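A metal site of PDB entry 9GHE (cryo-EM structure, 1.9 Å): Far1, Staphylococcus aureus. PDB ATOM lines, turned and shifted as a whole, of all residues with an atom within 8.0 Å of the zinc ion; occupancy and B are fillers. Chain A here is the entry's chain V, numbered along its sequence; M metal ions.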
ATOM      1  N   PHE A 119      24.438   1.457   6.475  1.00  0.00           N
ATOM      2  CA  PHE A 119      24.646   0.369   7.420  1.00  0.00           C
ATOM      3  C   PHE A 119      26.126   0.007   7.404  1.00  0.00           C
ATOM      4  O   PHE A 119      26.815   0.307   6.432  1.00  0.00           O
ATOM      5  CB  PHE A 119      23.772  -0.838   7.051  1.00  0.00           C
ATOM      6  CG  PHE A 119      24.171  -1.530   5.755  1.00  0.00           C
ATOM      7  CD1 PHE A 119      23.631  -1.136   4.543  1.00  0.00           C
ATOM      8  CD2 PHE A 119      25.077  -2.587   5.760  1.00  0.00           C
ATOM      9  CE1 PHE A 119      24.002  -1.766   3.366  1.00  0.00           C
ATOM     10  CE2 PHE A 119      25.448  -3.218   4.583  1.00  0.00           C
ATOM     11  CZ  PHE A 119      24.902  -2.803   3.382  1.00  0.00           C
ATOM     12  N   GLY A 155      25.078 -11.356  -9.607  1.00  0.00           N
ATOM     13  CA  GLY A 155      23.634 -11.310  -9.443  1.00  0.00           C
ATOM     14  C   GLY A 155      23.186  -9.969  -8.874  1.00  0.00           C
ATOM     15  O   GLY A 155      24.022  -9.164  -8.459  1.00  0.00           O
ATOM     16  N   PHE A 156      21.872  -9.733  -8.866  1.00  0.00           N
ATOM     17  CA  PHE A 156      21.317  -8.547  -8.246  1.00  0.00           C
ATOM     18  C   PHE A 156      21.298  -8.733  -6.727  1.00  0.00           C
ATOM     19  O   PHE A 156      20.961  -9.815  -6.254  1.00  0.00           O
ATOM     20  CB  PHE A 156      19.927  -8.254  -8.820  1.00  0.00           C
ATOM     21  CG  PHE A 156      19.935  -7.619 -10.200  1.00  0.00           C
ATOM     22  CD1 PHE A 156      20.068  -8.395 -11.342  1.00  0.00           C
ATOM     23  CD2 PHE A 156      19.784  -6.247 -10.355  1.00  0.00           C
ATOM     24  CE1 PHE A 156      20.071  -7.820 -12.599  1.00  0.00           C
ATOM     25  CE2 PHE A 156      19.779  -5.667 -11.616  1.00  0.00           C
ATOM     26  CZ  PHE A 156      19.924  -6.453 -12.742  1.00  0.00           C
ATOM     27  N   CYS A 157      21.662  -7.676  -5.993  1.00  0.00           N
ATOM     28  CA  CYS A 157      21.747  -7.724  -4.539  1.00  0.00           C
ATOM     29  C   CYS A 157      20.426  -7.273  -3.936  1.00  0.00           C
ATOM     30  O   CYS A 157      19.826  -6.308  -4.392  1.00  0.00           O
ATOM     31  CB  CYS A 157      22.910  -6.864  -4.077  1.00  0.00           C
ATOM     32  SG  CYS A 157      22.838  -6.304  -2.361  1.00  0.00           S
ATOM     33  N   THR A 158      19.989  -7.972  -2.874  1.00  0.00           N
ATOM     34  CA  THR A 158      18.700  -7.714  -2.263  1.00  0.00           C
ATOM     35  C   THR A 158      18.682  -6.332  -1.623  1.00  0.00           C
ATOM     36  O   THR A 158      17.655  -5.649  -1.639  1.00  0.00           O
ATOM     37  CB  THR A 158      18.382  -8.793  -1.225  1.00  0.00           C
ATOM     38  OG1 THR A 158      18.553 -10.047  -1.887  1.00  0.00           O
ATOM     39  CG2 THR A 158      16.967  -8.685  -0.694  1.00  0.00           C
ATOM     40  N   ILE A 159      19.814  -5.921  -1.041  1.00  0.00           N
ATOM     41  CA  ILE A 159      19.871  -4.680  -0.287  1.00  0.00           C
ATOM     42  C   ILE A 159      19.823  -3.492  -1.245  1.00  0.00           C
ATOM     43  O   ILE A 159      18.985  -2.606  -1.066  1.00  0.00           O
ATOM     44  CB  ILE A 159      21.101  -4.630   0.652  1.00  0.00           C
ATOM     45  CG1 ILE A 159      21.085  -5.796   1.650  1.00  0.00           C
ATOM     46  CG2 ILE A 159      21.186  -3.273   1.359  1.00  0.00           C
ATOM     47  CD1 ILE A 159      22.291  -5.862   2.562  1.00  0.00           C
ATOM     48  N   CYS A 160      20.687  -3.475  -2.266  1.00  0.00           N
ATOM     49  CA  CYS A 160      20.827  -2.300  -3.117  1.00  0.00           C
ATOM     50  C   CYS A 160      20.088  -2.452  -4.445  1.00  0.00           C
ATOM     51  O   CYS A 160      19.920  -1.454  -5.153  1.00  0.00           O
ATOM     52  CB  CYS A 160      22.283  -1.933  -3.336  1.00  0.00           C
ATOM     53  SG  CYS A 160      23.286  -3.193  -4.172  1.00  0.00           S
ATOM     54  N   ASN A 161      19.657  -3.674  -4.791  1.00  0.00           N
ATOM     55  CA  ASN A 161      18.891  -3.916  -6.012  1.00  0.00           C
ATOM     56  C   ASN A 161      19.716  -3.572  -7.248  1.00  0.00           C
ATOM     57  O   ASN A 161      19.162  -3.108  -8.244  1.00  0.00           O
ATOM     58  CB  ASN A 161      17.559  -3.162  -6.003  1.00  0.00           C
ATOM     59  CG  ASN A 161      16.674  -3.548  -4.845  1.00  0.00           C
ATOM     60  OD1 ASN A 161      16.985  -4.496  -4.109  1.00  0.00           O
ATOM     61  ND2 ASN A 161      15.575  -2.834  -4.668  1.00  0.00           N
ATOM     62  N   LYS A 162      21.028  -3.799  -7.177  1.00  0.00           N
ATOM     63  CA  LYS A 162      21.921  -3.561  -8.297  1.00  0.00           C
ATOM     64  C   LYS A 162      22.684  -4.853  -8.615  1.00  0.00           C
ATOM     65  O   LYS A 162      23.040  -5.595  -7.705  1.00  0.00           O
ATOM     66  CB  LYS A 162      22.943  -2.457  -7.986  1.00  0.00           C
ATOM     67  CG  LYS A 162      22.367  -1.132  -7.500  1.00  0.00           C
ATOM     68  CD  LYS A 162      21.422  -0.441  -8.477  1.00  0.00           C
ATOM     69  CE  LYS A 162      20.916   0.874  -7.971  1.00  0.00           C
ATOM     70  NZ  LYS A 162      20.139   0.746  -6.737  1.00  0.00           N
ATOM     71  N   GLU A 163      22.919  -5.107  -9.910  1.00  0.00           N
ATOM     72  CA  GLU A 163      23.712  -6.246 -10.324  1.00  0.00           C
ATOM     73  C   GLU A 163      25.144  -6.017  -9.865  1.00  0.00           C
ATOM     74  O   GLU A 163      25.736  -4.982 -10.173  1.00  0.00           O
ATOM     75  CB  GLU A 163      23.617  -6.462 -11.844  1.00  0.00           C
ATOM     76  CG  GLU A 163      23.910  -7.889 -12.276  1.00  0.00           C
ATOM     77  CD  GLU A 163      23.527  -8.216 -13.711  1.00  0.00           C
ATOM     78  OE1 GLU A 163      23.165  -7.289 -14.463  1.00  0.00           O
ATOM     79  OE2 GLU A 163      23.590  -9.412 -14.081  1.00  0.00           O
ATOM     80  N   SER A 164      25.689  -6.979  -9.112  1.00  0.00           N
ATOM     81  CA  SER A 164      26.972  -6.826  -8.455  1.00  0.00           C
ATOM     82  C   SER A 164      27.567  -8.193  -8.128  1.00  0.00           C
ATOM     83  O   SER A 164      26.947  -9.221  -8.410  1.00  0.00           O
ATOM     84  CB  SER A 164      26.840  -5.971  -7.212  1.00  0.00           C
ATOM     85  OG  SER A 164      26.326  -4.685  -7.514  1.00  0.00           O
ATOM     86  N   ASN A 165      28.770  -8.202  -7.532  1.00  0.00           N
ATOM     87  CA  ASN A 165      29.345  -9.426  -7.004  1.00  0.00           C
ATOM     88  C   ASN A 165      28.667  -9.732  -5.673  1.00  0.00           C
ATOM     89  O   ASN A 165      28.813  -8.967  -4.715  1.00  0.00           O
ATOM     90  CB  ASN A 165      30.861  -9.319  -6.823  1.00  0.00           C
ATOM     91  CG  ASN A 165      31.535  -8.698  -8.021  1.00  0.00           C
ATOM     92  OD1 ASN A 165      31.360  -9.176  -9.149  1.00  0.00           O
ATOM     93  ND2 ASN A 165      32.292  -7.633  -7.804  1.00  0.00           N
ATOM     94  N   VAL A 166      27.921 -10.844  -5.614  1.00  0.00           N
ATOM     95  CA  VAL A 166      27.091 -11.148  -4.464  1.00  0.00           C
ATOM     96  C   VAL A 166      27.411 -12.556  -3.969  1.00  0.00           C
ATOM     97  O   VAL A 166      27.982 -13.367  -4.704  1.00  0.00           O
ATOM     98  CB  VAL A 166      25.596 -10.993  -4.795  1.00  0.00           C
ATOM     99  CG1 VAL A 166      25.236  -9.533  -5.089  1.00  0.00           C
ATOM    100  CG2 VAL A 166      25.153 -11.889  -5.942  1.00  0.00           C
ATOM    101  N   TYR A 187      20.791 -13.256  -1.621  1.00  0.00           N
ATOM    102  CA  TYR A 187      22.032 -12.827  -2.241  1.00  0.00           C
ATOM    103  C   TYR A 187      22.237 -11.339  -1.982  1.00  0.00           C
ATOM    104  O   TYR A 187      21.373 -10.525  -2.282  1.00  0.00           O
ATOM    105  CB  TYR A 187      22.038 -13.178  -3.734  1.00  0.00           C
ATOM    106  CG  TYR A 187      22.407 -14.623  -4.022  1.00  0.00           C
ATOM    107  CD1 TYR A 187      21.445 -15.625  -4.058  1.00  0.00           C
ATOM    108  CD2 TYR A 187      23.728 -14.993  -4.247  1.00  0.00           C
ATOM    109  CE1 TYR A 187      21.783 -16.945  -4.319  1.00  0.00           C
ATOM    110  CE2 TYR A 187      24.078 -16.308  -4.502  1.00  0.00           C
ATOM    111  CZ  TYR A 187      23.102 -17.293  -4.542  1.00  0.00           C
ATOM    112  OH  TYR A 187      23.438 -18.583  -4.789  1.00  0.00           O
ATOM    113  N   ILE A 188      23.391 -10.995  -1.390  1.00  0.00           N
ATOM    114  CA  ILE A 188      23.740  -9.617  -1.092  1.00  0.00           C
ATOM    115  C   ILE A 188      25.204  -9.397  -1.486  1.00  0.00           C
ATOM    116  O   ILE A 188      25.972 -10.352  -1.573  1.00  0.00           O
ATOM    117  CB  ILE A 188      23.491  -9.293   0.385  1.00  0.00           C
ATOM    118  CG1 ILE A 188      24.387 -10.119   1.319  1.00  0.00           C
ATOM    119  CG2 ILE A 188      22.003  -9.456   0.732  1.00  0.00           C
ATOM    120  CD1 ILE A 188      24.251  -9.767   2.786  1.00  0.00           C
ATOM    121  N   CYS A 189      25.582  -8.123  -1.701  1.00  0.00           N
ATOM    122  CA  CYS A 189      26.949  -7.780  -2.054  1.00  0.00           C
ATOM    123  C   CYS A 189      27.907  -8.303  -0.991  1.00  0.00           C
ATOM    124  O   CYS A 189      27.662  -8.155   0.196  1.00  0.00           O
ATOM    125  CB  CYS A 189      27.141  -6.263  -2.152  1.00  0.00           C
ATOM    126  SG  CYS A 189      26.202  -5.428  -3.449  1.00  0.00           S
ATOM    127  N   ARG A 190      29.003  -8.929  -1.445  1.00  0.00           N
ATOM    128  CA  ARG A 190      30.006  -9.455  -0.529  1.00  0.00           C
ATOM    129  C   ARG A 190      30.705  -8.290   0.176  1.00  0.00           C
ATOM    130  O   ARG A 190      31.011  -8.381   1.370  1.00  0.00           O
ATOM    131  CB  ARG A 190      31.033 -10.337  -1.253  1.00  0.00           C
ATOM    132  CG  ARG A 190      31.795 -11.244  -0.292  1.00  0.00           C
ATOM    133  CD  ARG A 190      32.959 -11.956  -0.939  1.00  0.00           C
ATOM    134  NE  ARG A 190      33.483 -12.990  -0.040  1.00  0.00           N
ATOM    135  CZ  ARG A 190      32.835 -14.107   0.308  1.00  0.00           C
ATOM    136  NH1 ARG A 190      31.773 -14.501  -0.373  1.00  0.00           N
ATOM    137  NH2 ARG A 190      33.279 -14.835   1.315  1.00  0.00           N
ATOM    138  N   ASP A 191      30.939  -7.196  -0.565  1.00  0.00           N
ATOM    139  CA  ASP A 191      31.509  -5.973   0.000  1.00  0.00           C
ATOM    140  C   ASP A 191      30.368  -5.033   0.392  1.00  0.00           C
ATOM    141  O   ASP A 191      29.680  -4.504  -0.480  1.00  0.00           O
ATOM    142  CB  ASP A 191      32.462  -5.304  -0.973  1.00  0.00           C
ATOM    143  CG  ASP A 191      33.193  -4.080  -0.456  1.00  0.00           C
ATOM    144  OD1 ASP A 191      33.091  -3.792   0.751  1.00  0.00           O
ATOM    145  OD2 ASP A 191      33.856  -3.406  -1.284  1.00  0.00           O
ATOM    146  N   SER A 192      30.198  -4.829   1.699  1.00  0.00           N
ATOM    147  CA  SER A 192      29.147  -3.963   2.220  1.00  0.00           C
ATOM    148  C   SER A 192      29.437  -2.498   1.926  1.00  0.00           C
ATOM    149  O   SER A 192      28.498  -1.709   1.789  1.00  0.00           O
ATOM    150  CB  SER A 192      28.959  -4.185   3.701  1.00  0.00           C
ATOM    151  OG  SER A 192      28.523  -5.511   3.970  1.00  0.00           O
ATOM    152  N   HIS A 194      30.875  -1.225  -0.811  1.00  0.00           N
ATOM    153  CA  HIS A 194      30.397  -1.009  -2.165  1.00  0.00           C
ATOM    154  C   HIS A 194      28.873  -1.000  -2.177  1.00  0.00           C
ATOM    155  O   HIS A 194      28.260  -0.184  -2.849  1.00  0.00           O
ATOM    156  CB  HIS A 194      30.968  -2.071  -3.126  1.00  0.00           C
ATOM    157  CG  HIS A 194      30.567  -1.872  -4.547  1.00  0.00           C
ATOM    158  ND1 HIS A 194      30.364  -0.632  -5.102  1.00  0.00           N
ATOM    159  CD2 HIS A 194      30.336  -2.755  -5.528  1.00  0.00           C
ATOM    160  CE1 HIS A 194      30.024  -0.770  -6.378  1.00  0.00           C
ATOM    161  NE2 HIS A 194      29.999  -2.051  -6.656  1.00  0.00           N
ATOM    162  N   CYS A 195      28.272  -1.925  -1.402  1.00  0.00           N
ATOM    163  CA  CYS A 195      26.827  -2.018  -1.291  1.00  0.00           C
ATOM    164  C   CYS A 195      26.234  -0.692  -0.791  1.00  0.00           C
ATOM    165  O   CYS A 195      25.231  -0.230  -1.328  1.00  0.00           O
ATOM    166  CB  CYS A 195      26.446  -3.163  -0.359  1.00  0.00           C
ATOM    167  SG  CYS A 195      24.682  -3.576  -0.376  1.00  0.00           S
ATOM    168  N   ASN A 196      26.862  -0.115   0.239  1.00  0.00           N
ATOM    169  CA  ASN A 196      26.393   1.120   0.850  1.00  0.00           C
ATOM    170  C   ASN A 196      26.416   2.258  -0.171  1.00  0.00           C
ATOM    171  O   ASN A 196      25.508   3.094  -0.177  1.00  0.00           O
ATOM    172  CB  ASN A 196      27.179   1.470   2.096  1.00  0.00           C
ATOM    173  CG  ASN A 196      26.595   0.833   3.344  1.00  0.00           C
ATOM    174  OD1 ASN A 196      25.522   1.239   3.798  1.00  0.00           O
ATOM    175  ND2 ASN A 196      27.285  -0.154   3.904  1.00  0.00           N
ATOM    176  N   LYS A 197      27.452   2.288  -1.012  1.00  0.00           N
ATOM    177  CA  LYS A 197      27.575   3.305  -2.049  1.00  0.00           C
ATOM    178  C   LYS A 197      26.445   3.155  -3.068  1.00  0.00           C
ATOM    179  O   LYS A 197      25.904   4.158  -3.535  1.00  0.00           O
ATOM    180  CB  LYS A 197      28.926   3.212  -2.762  1.00  0.00           C
ATOM    181  CG  LYS A 197      30.154   3.390  -1.871  1.00  0.00           C
ATOM    182  CD  LYS A 197      31.452   2.943  -2.529  1.00  0.00           C
ATOM    183  CE  LYS A 197      32.623   3.053  -1.607  1.00  0.00           C
ATOM    184  NZ  LYS A 197      33.843   2.488  -2.184  1.00  0.00           N
ATOM    185  N   GLN A 198      26.111   1.903  -3.396  1.00  0.00           N
ATOM    186  CA  GLN A 198      25.079   1.617  -4.380  1.00  0.00           C
ATOM    187  C   GLN A 198      23.687   1.932  -3.829  1.00  0.00           C
ATOM    188  O   GLN A 198      22.802   2.289  -4.595  1.00  0.00           O
ATOM    189  CB  GLN A 198      25.153   0.149  -4.818  1.00  0.00           C
ATOM    190  CG  GLN A 198      26.417  -0.215  -5.590  1.00  0.00           C
ATOM    191  CD  GLN A 198      26.486  -1.675  -5.974  1.00  0.00           C
ATOM    192  OE1 GLN A 198      26.568  -2.017  -7.164  1.00  0.00           O
ATOM    193  NE2 GLN A 198      26.464  -2.556  -4.992  1.00  0.00           N
ATOM    194  N   LEU A 199      23.508   1.791  -2.511  1.00  0.00           N
ATOM    195  CA  LEU A 199      22.209   1.962  -1.895  1.00  0.00           C
ATOM    196  C   LEU A 199      21.783   3.426  -1.985  1.00  0.00           C
ATOM    197  O   LEU A 199      22.545   4.307  -1.616  1.00  0.00           O
ATOM    198  CB  LEU A 199      22.251   1.495  -0.434  1.00  0.00           C
ATOM    199  CG  LEU A 199      20.897   1.420   0.287  1.00  0.00           C
ATOM    200  CD1 LEU A 199      19.979   0.421  -0.406  1.00  0.00           C
ATOM    201  CD2 LEU A 199      21.091   1.042   1.742  1.00  0.00           C
ATOM    202  N   GLN A 204      14.943  -0.007   1.212  1.00  0.00           N
ATOM    203  CA  GLN A 204      15.343  -1.255   0.579  1.00  0.00           C
ATOM    204  C   GLN A 204      16.095  -2.135   1.572  1.00  0.00           C
ATOM    205  O   GLN A 204      15.861  -3.343   1.619  1.00  0.00           O
ATOM    206  CB  GLN A 204      16.213  -1.014  -0.662  1.00  0.00           C
ATOM    207  CG  GLN A 204      15.554  -0.146  -1.726  1.00  0.00           C
ATOM    208  CD  GLN A 204      16.450   0.114  -2.918  1.00  0.00           C
ATOM    209  OE1 GLN A 204      17.579  -0.395  -3.007  1.00  0.00           O
ATOM    210  NE2 GLN A 204      15.958   0.916  -3.859  1.00  0.00           N
HETATM  211 ZN    ZN M   1      24.285  -4.478  -2.503  1.00  0.00          ZN
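The side-chain amide oxygen (OE1) of Gln 198 sits at hydrogen-bond distance from a ring nitrogen (NE2) of His 194 (3.5 Å).
The side-chain sulfur of Cys 157 lies close to the backbone NH of Ile 159.
The side-chain amide oxygen (OE1) of Gln 198 sits at hydrogen-bond distance from the side-chain hydroxyl (OG) of Ser 164, at 2.7 Å.
The side-chain sulfur (SG) of Cys 189 sits close to the side-chain amide nitrogen (NE2) of Gln 198, at 3.3 Å.
The backbone carbonyl oxygen (O) of Cys 160 lies within hydrogen-bond range of the side-chain amino group (NZ) of Lys 162, 2.7 Å away.
N of Cys 157 sits at hydrogen-bond distance from O of Lys 162, at 3.0 Å.
O of Cys 160 lies close to OE1 of Gln 204 (3.3 Å).
SG of Cys 160 sits close to NE2 of Gln 198.
Gln 198 touches the zinc ion (NE2 to ZN, 3.8 Å).
Of the 26 residues printed, 5 come within 4 Å of the zinc ion.
The zinc ion is bound by SG of Cys 160 (2.3 Å), SG of Cys 157 (2.3 Å), SG of Cys 189 (2.3 Å) and SG of Cys 195 (2.3 Å).
The zinc ion has four donor atoms within binding distance.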
